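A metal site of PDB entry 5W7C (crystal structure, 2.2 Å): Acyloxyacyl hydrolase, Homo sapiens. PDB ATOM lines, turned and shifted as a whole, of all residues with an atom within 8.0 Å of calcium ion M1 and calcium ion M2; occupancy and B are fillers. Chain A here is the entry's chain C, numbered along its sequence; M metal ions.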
ATOM      1  N   PRO A  29     -26.082 -13.722   9.813  1.00  0.00           N
ATOM      2  CA  PRO A  29     -26.174 -13.179   8.457  1.00  0.00           C
ATOM      3  C   PRO A  29     -27.463 -13.592   7.755  1.00  0.00           C
ATOM      4  O   PRO A  29     -27.896 -14.744   7.848  1.00  0.00           O
ATOM      5  CB  PRO A  29     -24.942 -13.766   7.757  1.00  0.00           C
ATOM      6  CG  PRO A  29     -24.497 -14.912   8.614  1.00  0.00           C
ATOM      7  CD  PRO A  29     -24.876 -14.531  10.009  1.00  0.00           C
ATOM      8  N   LYS A  31     -27.643 -13.442   4.394  1.00  0.00           N
ATOM      9  CA  LYS A  31     -27.114 -14.181   3.240  1.00  0.00           C
ATOM     10  C   LYS A  31     -26.129 -15.218   3.769  1.00  0.00           C
ATOM     11  O   LYS A  31     -24.990 -14.885   4.113  1.00  0.00           O
ATOM     12  CB  LYS A  31     -26.487 -13.229   2.235  1.00  0.00           C
ATOM     13  CG  LYS A  31     -27.509 -12.669   1.260  1.00  0.00           C
ATOM     14  CD  LYS A  31     -26.961 -11.543   0.404  1.00  0.00           C
ATOM     15  CE  LYS A  31     -28.065 -10.934  -0.443  1.00  0.00           C
ATOM     16  NZ  LYS A  31     -27.526 -10.058  -1.529  1.00  0.00           N
ATOM     17  N   ASP A  32     -26.575 -16.469   3.825  1.00  0.00           N
ATOM     18  CA  ASP A  32     -25.849 -17.538   4.486  1.00  0.00           C
ATOM     19  C   ASP A  32     -26.418 -18.877   4.036  1.00  0.00           C
ATOM     20  O   ASP A  32     -27.226 -19.495   4.742  1.00  0.00           O
ATOM     21  CB  ASP A  32     -25.950 -17.386   6.012  1.00  0.00           C
ATOM     22  CG  ASP A  32     -25.068 -18.350   6.758  1.00  0.00           C
ATOM     23  OD1 ASP A  32     -24.127 -18.903   6.151  1.00  0.00           O
ATOM     24  OD2 ASP A  32     -25.313 -18.559   7.972  1.00  0.00           O
ATOM     25  N   VAL A  33     -26.017 -19.330   2.850  1.00  0.00           N
ATOM     26  CA  VAL A  33     -26.660 -20.478   2.220  1.00  0.00           C
ATOM     27  C   VAL A  33     -26.416 -21.743   3.040  1.00  0.00           C
ATOM     28  O   VAL A  33     -27.349 -22.512   3.315  1.00  0.00           O
ATOM     29  CB  VAL A  33     -26.177 -20.632   0.766  1.00  0.00           C
ATOM     30  CG1 VAL A  33     -26.746 -21.899   0.135  1.00  0.00           C
ATOM     31  CG2 VAL A  33     -26.576 -19.412  -0.044  1.00  0.00           C
ATOM     32  N   ASP A  34     -25.174 -21.985   3.429  1.00  0.00           N
ATOM     33  CA  ASP A  34     -24.844 -23.183   4.207  1.00  0.00           C
ATOM     34  C   ASP A  34     -25.136 -23.018   5.691  1.00  0.00           C
ATOM     35  O   ASP A  34     -24.942 -23.970   6.454  1.00  0.00           O
ATOM     36  CB  ASP A  34     -23.377 -23.563   3.996  1.00  0.00           C
ATOM     37  CG  ASP A  34     -22.423 -22.428   4.320  1.00  0.00           C
ATOM     38  OD1 ASP A  34     -22.800 -21.521   5.092  1.00  0.00           O
ATOM     39  OD2 ASP A  34     -21.289 -22.448   3.802  1.00  0.00           O
ATOM     40  N   SER A  35     -25.577 -21.832   6.130  1.00  0.00           N
ATOM     41  CA  SER A  35     -26.054 -21.633   7.502  1.00  0.00           C
ATOM     42  C   SER A  35     -24.954 -21.898   8.532  1.00  0.00           C
ATOM     43  O   SER A  35     -25.199 -22.471   9.589  1.00  0.00           O
ATOM     44  CB  SER A  35     -27.275 -22.486   7.796  1.00  0.00           C
ATOM     45  OG  SER A  35     -28.428 -22.011   7.119  1.00  0.00           O
ATOM     46  N   ASP A  36     -23.730 -21.462   8.237  1.00  0.00           N
ATOM     47  CA  ASP A  36     -22.646 -21.531   9.200  1.00  0.00           C
ATOM     48  C   ASP A  36     -22.364 -20.186   9.852  1.00  0.00           C
ATOM     49  O   ASP A  36     -21.371 -20.053  10.579  1.00  0.00           O
ATOM     50  CB  ASP A  36     -21.363 -22.075   8.550  1.00  0.00           C
ATOM     51  CG  ASP A  36     -20.922 -21.280   7.347  1.00  0.00           C
ATOM     52  OD1 ASP A  36     -21.307 -20.098   7.234  1.00  0.00           O
ATOM     53  OD2 ASP A  36     -20.176 -21.834   6.517  1.00  0.00           O
ATOM     54  N   LYS A  37     -23.223 -19.187   9.623  1.00  0.00           N
ATOM     55  CA  LYS A  37     -23.172 -17.865  10.243  1.00  0.00           C
ATOM     56  C   LYS A  37     -22.086 -16.988   9.652  1.00  0.00           C
ATOM     57  O   LYS A  37     -21.818 -15.908  10.198  1.00  0.00           O
ATOM     58  CB  LYS A  37     -22.980 -17.953  11.759  1.00  0.00           C
ATOM     59  CG  LYS A  37     -24.002 -18.842  12.459  1.00  0.00           C
ATOM     60  CD  LYS A  37     -23.924 -18.712  13.969  1.00  0.00           C
ATOM     61  CE  LYS A  37     -24.768 -19.757  14.670  1.00  0.00           C
ATOM     62  NZ  LYS A  37     -23.916 -20.658  15.507  1.00  0.00           N
ATOM     63  N   TYR A  38     -21.454 -17.392   8.551  1.00  0.00           N
ATOM     64  CA  TYR A  38     -20.530 -16.541   7.814  1.00  0.00           C
ATOM     65  C   TYR A  38     -21.114 -16.273   6.425  1.00  0.00           C
ATOM     66  O   TYR A  38     -21.758 -17.155   5.842  1.00  0.00           O
ATOM     67  CB  TYR A  38     -19.146 -17.177   7.711  1.00  0.00           C
ATOM     68  CG  TYR A  38     -18.458 -17.337   9.044  1.00  0.00           C
ATOM     69  CD1 TYR A  38     -17.612 -16.351   9.529  1.00  0.00           C
ATOM     70  CD2 TYR A  38     -18.665 -18.456   9.825  1.00  0.00           C
ATOM     71  CE1 TYR A  38     -16.981 -16.487  10.758  1.00  0.00           C
ATOM     72  CE2 TYR A  38     -18.032 -18.601  11.051  1.00  0.00           C
ATOM     73  CZ  TYR A  38     -17.197 -17.621  11.509  1.00  0.00           C
ATOM     74  OH  TYR A  38     -16.564 -17.754  12.729  1.00  0.00           O
ATOM     75  N   SER A  39     -20.892 -15.064   5.917  1.00  0.00           N
ATOM     76  CA  SER A  39     -21.621 -14.579   4.762  1.00  0.00           C
ATOM     77  C   SER A  39     -20.659 -14.133   3.667  1.00  0.00           C
ATOM     78  O   SER A  39     -19.471 -13.887   3.906  1.00  0.00           O
ATOM     79  CB  SER A  39     -22.535 -13.399   5.147  1.00  0.00           C
ATOM     80  OG  SER A  39     -23.257 -12.914   4.037  1.00  0.00           O
ATOM     81  N   VAL A  40     -21.195 -14.057   2.441  1.00  0.00           N
ATOM     82  CA  VAL A  40     -20.486 -13.457   1.313  1.00  0.00           C
ATOM     83  C   VAL A  40     -20.890 -12.007   1.103  1.00  0.00           C
ATOM     84  O   VAL A  40     -20.216 -11.286   0.356  1.00  0.00           O
ATOM     85  CB  VAL A  40     -20.728 -14.257   0.011  1.00  0.00           C
ATOM     86  CG1 VAL A  40     -20.246 -15.693   0.170  1.00  0.00           C
ATOM     87  CG2 VAL A  40     -22.196 -14.212  -0.393  1.00  0.00           C
ATOM     88  N   GLY A  51     -15.602 -12.938   9.518  1.00  0.00           N
ATOM     89  CA  GLY A  51     -14.811 -13.280   8.348  1.00  0.00           C
ATOM     90  C   GLY A  51     -15.691 -13.678   7.177  1.00  0.00           C
ATOM     91  O   GLY A  51     -16.713 -14.355   7.342  1.00  0.00           O
ATOM     92  N   ARG A  52     -15.292 -13.252   5.989  1.00  0.00           N
ATOM     93  CA  ARG A  52     -16.029 -13.599   4.774  1.00  0.00           C
ATOM     94  C   ARG A  52     -15.965 -15.106   4.543  1.00  0.00           C
ATOM     95  O   ARG A  52     -14.900 -15.719   4.630  1.00  0.00           O
ATOM     96  CB  ARG A  52     -15.434 -12.851   3.582  1.00  0.00           C
ATOM     97  CG  ARG A  52     -16.225 -12.957   2.295  1.00  0.00           C
ATOM     98  CD  ARG A  52     -15.441 -12.332   1.152  1.00  0.00           C
ATOM     99  NE  ARG A  52     -16.304 -11.869   0.064  1.00  0.00           N
ATOM    100  CZ  ARG A  52     -16.404 -10.609  -0.364  1.00  0.00           C
ATOM    101  NH1 ARG A  52     -15.681  -9.644   0.191  1.00  0.00           N
ATOM    102  NH2 ARG A  52     -17.230 -10.322  -1.362  1.00  0.00           N
ATOM    103  N   ASP A  53     -17.119 -15.695   4.260  1.00  0.00           N
ATOM    104  CA  ASP A  53     -17.189 -17.124   3.969  1.00  0.00           C
ATOM    105  C   ASP A  53     -16.593 -17.399   2.600  1.00  0.00           C
ATOM    106  O   ASP A  53     -17.107 -16.924   1.581  1.00  0.00           O
ATOM    107  CB  ASP A  53     -18.639 -17.609   4.028  1.00  0.00           C
ATOM    108  CG  ASP A  53     -18.754 -19.118   4.100  1.00  0.00           C
ATOM    109  OD1 ASP A  53     -17.729 -19.822   3.928  1.00  0.00           O
ATOM    110  OD2 ASP A  53     -19.881 -19.615   4.322  1.00  0.00           O
ATOM    111  N   CYS A  54     -15.482 -18.159   2.560  1.00  0.00           N
ATOM    112  CA  CYS A  54     -14.855 -18.484   1.290  1.00  0.00           C
ATOM    113  C   CYS A  54     -15.628 -19.540   0.507  1.00  0.00           C
ATOM    114  O   CYS A  54     -15.373 -19.698  -0.690  1.00  0.00           O
ATOM    115  CB  CYS A  54     -13.415 -18.963   1.527  1.00  0.00           C
ATOM    116  SG  CYS A  54     -13.226 -20.282   2.761  1.00  0.00           S
ATOM    117  N   ASN A  55     -16.547 -20.257   1.151  1.00  0.00           N
ATOM    118  CA  ASN A  55     -17.392 -21.224   0.445  1.00  0.00           C
ATOM    119  C   ASN A  55     -18.747 -21.239   1.146  1.00  0.00           C
ATOM    120  O   ASN A  55     -18.953 -21.980   2.110  1.00  0.00           O
ATOM    121  CB  ASN A  55     -16.774 -22.614   0.414  1.00  0.00           C
ATOM    122  CG  ASN A  55     -17.408 -23.504  -0.636  1.00  0.00           C
ATOM    123  OD1 ASN A  55     -18.586 -23.340  -0.949  1.00  0.00           O
ATOM    124  ND2 ASN A  55     -16.639 -24.442  -1.180  1.00  0.00           N
ATOM    125  N   ASP A  56     -19.682 -20.440   0.634  1.00  0.00           N
ATOM    126  CA  ASP A  56     -21.015 -20.360   1.209  1.00  0.00           C
ATOM    127  C   ASP A  56     -21.869 -21.575   0.884  1.00  0.00           C
ATOM    128  O   ASP A  56     -23.054 -21.589   1.246  1.00  0.00           O
ATOM    129  CB  ASP A  56     -21.721 -19.080   0.735  1.00  0.00           C
ATOM    130  CG  ASP A  56     -22.896 -18.700   1.616  1.00  0.00           C
ATOM    131  OD1 ASP A  56     -22.832 -18.923   2.837  1.00  0.00           O
ATOM    132  OD2 ASP A  56     -23.897 -18.177   1.069  1.00  0.00           O
ATOM    133  N   SER A  57     -21.313 -22.578   0.210  1.00  0.00           N
ATOM    134  CA  SER A  57     -22.015 -23.829  -0.069  1.00  0.00           C
ATOM    135  C   SER A  57     -21.393 -25.018   0.655  1.00  0.00           C
ATOM    136  O   SER A  57     -21.568 -26.157   0.220  1.00  0.00           O
ATOM    137  CB  SER A  57     -22.049 -24.086  -1.578  1.00  0.00           C
ATOM    138  OG  SER A  57     -22.711 -23.037  -2.262  1.00  0.00           O
ATOM    139  N   ASP A  58     -20.662 -24.765   1.738  1.00  0.00           N
ATOM    140  CA  ASP A  58     -20.059 -25.835   2.520  1.00  0.00           C
ATOM    141  C   ASP A  58     -20.035 -25.386   3.984  1.00  0.00           C
ATOM    142  O   ASP A  58     -19.190 -24.566   4.367  1.00  0.00           O
ATOM    143  CB  ASP A  58     -18.659 -26.163   2.016  1.00  0.00           C
ATOM    144  CG  ASP A  58     -18.106 -27.454   2.612  1.00  0.00           C
ATOM    145  OD1 ASP A  58     -18.574 -27.848   3.696  1.00  0.00           O
ATOM    146  OD2 ASP A  58     -17.211 -28.067   1.983  1.00  0.00           O
ATOM    147  N   GLU A  59     -20.960 -25.920   4.775  1.00  0.00           N
ATOM    148  CA  GLU A  59     -21.017 -25.587   6.190  1.00  0.00           C
ATOM    149  C   GLU A  59     -19.744 -25.961   6.933  1.00  0.00           C
ATOM    150  O   GLU A  59     -19.487 -25.426   8.006  1.00  0.00           O
ATOM    151  CB  GLU A  59     -22.211 -26.286   6.848  1.00  0.00           C
ATOM    152  CG  GLU A  59     -22.057 -27.793   6.944  1.00  0.00           C
ATOM    153  CD  GLU A  59     -23.338 -28.495   7.373  1.00  0.00           C
ATOM    154  OE1 GLU A  59     -24.062 -27.932   8.233  1.00  0.00           O
ATOM    155  OE2 GLU A  59     -23.624 -29.590   6.860  1.00  0.00           O
ATOM    156  N   SER A  60     -18.954 -26.880   6.379  1.00  0.00           N
ATOM    157  CA  SER A  60     -17.696 -27.285   6.987  1.00  0.00           C
ATOM    158  C   SER A  60     -16.537 -26.390   6.594  1.00  0.00           C
ATOM    159  O   SER A  60     -15.383 -26.695   6.929  1.00  0.00           O
ATOM    160  CB  SER A  60     -17.374 -28.735   6.612  1.00  0.00           C
ATOM    161  OG  SER A  60     -18.380 -29.623   7.089  1.00  0.00           O
ATOM    162  N   VAL A  61     -16.801 -25.283   5.899  1.00  0.00           N
ATOM    163  CA  VAL A  61     -15.787 -24.327   5.491  1.00  0.00           C
ATOM    164  C   VAL A  61     -16.185 -22.963   6.024  1.00  0.00           C
ATOM    165  O   VAL A  61     -17.242 -22.429   5.652  1.00  0.00           O
ATOM    166  CB  VAL A  61     -15.615 -24.287   3.962  1.00  0.00           C
ATOM    167  CG1 VAL A  61     -14.600 -23.224   3.558  1.00  0.00           C
ATOM    168  CG2 VAL A  61     -15.188 -25.658   3.445  1.00  0.00           C
ATOM    169  N   TYR A  62     -15.359 -22.386   6.884  1.00  0.00           N
ATOM    170  CA  TYR A  62     -15.621 -21.084   7.462  1.00  0.00           C
ATOM    171  C   TYR A  62     -14.382 -20.640   8.238  1.00  0.00           C
ATOM    172  O   TYR A  62     -13.552 -21.480   8.601  1.00  0.00           O
ATOM    173  CB  TYR A  62     -16.843 -21.116   8.396  1.00  0.00           C
ATOM    174  CG  TYR A  62     -16.798 -22.208   9.444  1.00  0.00           C
ATOM    175  CD1 TYR A  62     -16.093 -22.032  10.625  1.00  0.00           C
ATOM    176  CD2 TYR A  62     -17.449 -23.414   9.248  1.00  0.00           C
ATOM    177  CE1 TYR A  62     -16.038 -23.021  11.581  1.00  0.00           C
ATOM    178  CE2 TYR A  62     -17.413 -24.407  10.198  1.00  0.00           C
ATOM    179  CZ  TYR A  62     -16.706 -24.215  11.363  1.00  0.00           C
ATOM    180  OH  TYR A  62     -16.670 -25.207  12.312  1.00  0.00           O
ATOM    181  N   PRO A  63     -14.246 -19.345   8.500  1.00  0.00           N
ATOM    182  CA  PRO A  63     -13.085 -18.867   9.268  1.00  0.00           C
ATOM    183  C   PRO A  63     -13.029 -19.492  10.653  1.00  0.00           C
ATOM    184  O   PRO A  63     -14.055 -19.703  11.303  1.00  0.00           O
ATOM    185  CB  PRO A  63     -13.300 -17.356   9.332  1.00  0.00           C
ATOM    186  CG  PRO A  63     -14.177 -17.037   8.170  1.00  0.00           C
ATOM    187  CD  PRO A  63     -15.062 -18.227   7.997  1.00  0.00           C
ATOM    188  N   GLN A  74      -8.998 -27.899  -0.566  1.00  0.00           N
ATOM    189  CA  GLN A  74      -9.836 -26.739  -0.310  1.00  0.00           C
ATOM    190  C   GLN A  74      -9.275 -25.957   0.869  1.00  0.00           C
ATOM    191  O   GLN A  74      -8.728 -26.542   1.815  1.00  0.00           O
ATOM    192  CB  GLN A  74     -11.287 -27.136  -0.026  1.00  0.00           C
ATOM    193  CG  GLN A  74     -12.291 -26.614  -1.041  1.00  0.00           C
ATOM    194  CD  GLN A  74     -13.667 -26.377  -0.454  1.00  0.00           C
ATOM    195  OE1 GLN A  74     -14.152 -25.254  -0.417  1.00  0.00           O
ATOM    196  NE2 GLN A  74     -14.304 -27.450   0.007  1.00  0.00           N
ATOM    197  N   SER A  76     -10.220 -24.691   3.894  1.00  0.00           N
ATOM    198  CA  SER A  76     -11.355 -24.971   4.765  1.00  0.00           C
ATOM    199  C   SER A  76     -11.568 -23.922   5.844  1.00  0.00           C
ATOM    200  O   SER A  76     -12.630 -23.928   6.490  1.00  0.00           O
ATOM    201  CB  SER A  76     -11.187 -26.350   5.419  1.00  0.00           C
ATOM    202  OG  SER A  76     -10.116 -26.348   6.348  1.00  0.00           O
ATOM    203  N   CYS A  78     -10.727 -20.428   5.201  1.00  0.00           N
ATOM    204  CA  CYS A  78     -10.840 -19.119   4.547  1.00  0.00           C
ATOM    205  C   CYS A  78      -9.676 -18.196   4.872  1.00  0.00           C
ATOM    206  O   CYS A  78      -9.805 -16.969   4.729  1.00  0.00           O
ATOM    207  CB  CYS A  78     -12.151 -18.435   4.934  1.00  0.00           C
ATOM    208  SG  CYS A  78     -13.640 -19.398   4.548  1.00  0.00           S
HETATM  209 CA    CA M   1     -19.138 -21.972   4.501  1.00  0.00          CA
HETATM  210 CA    CA M   2     -22.030 -19.382   5.171  1.00  0.00          CA
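OH of Tyr 38 lies within hydrogen-bond range of O of Pro 63.
The side-chain carboxylate (OD2) of Asp 32 lies within hydrogen-bond range of the backbone NH (N) of Lys 37 (2.7 Å).
The backbone carbonyl oxygen of Ser 39 sits at hydrogen-bond distance from the backbone NH of Asp 53, at 3.0 Å.
The side-chain sulfur (SG) of Cys 54 forms a disulfide with the side-chain sulfur (SG) of Cys 78 (2.0 Å).
The side-chain carboxylate (OD1) of Asp 58 lies within hydrogen-bond range of the backbone NH (N) of Ser 60 (2.9 Å).
The side-chain amide oxygen of Asn 55 lies close to the backbone NH of Ser 57 (3.1 Å).
OD2 of Asp 56 lies within hydrogen-bond range of N of Val 33, 3.0 Å away.
The side-chain amide oxygen (OE1) of Gln 74 lies within hydrogen-bond range of the side-chain amide nitrogen (ND2) of Asn 55 (2.7 Å).
Six residues have an atom within 4 Å of calcium ion M1: Asp 34, Asp 36, Asp 53, Asn 55, Asp 58 and Val 61.
Of the 27 residues printed, 6 come within 4 Å of calcium ion M2.
The nearest printed residue that does not touch calcium ion M2 is Ser 35 (4.4 Å).
Calcium ion M1 is bound by the backbone carbonyl oxygen (O) of Val 61 (2.3 Å).
The side-chain carboxylate (OD2) of Asp 36 is bound to calcium ion M1, 2.3 Å away.
Calcium ion M1 is bound by the side-chain carboxylate (OD2) of Asp 34 (2.3 Å).
O of Asn 55 is bound to calcium ion M1 (2.4 Å).
Calcium ion M1 is bound by the side-chain carboxylate (OD2) of Asp 53.
O of Asp 58 is bound to calcium ion M1, 2.6 Å away.
The side-chain carboxylate (OD1) of Asp 53 binds calcium ion M1, at 2.6 Å.
Calcium ion M2 is bound by OD1 of Asp 34 (2.3 Å), OD1 of Asp 36 (2.3 Å), OD2 of Asp 53 (2.3 Å), O of Tyr 38 (2.3 Å), OD1 of Asp 32 (2.4 Å) and OD1 of Asp 56 (2.5 Å).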
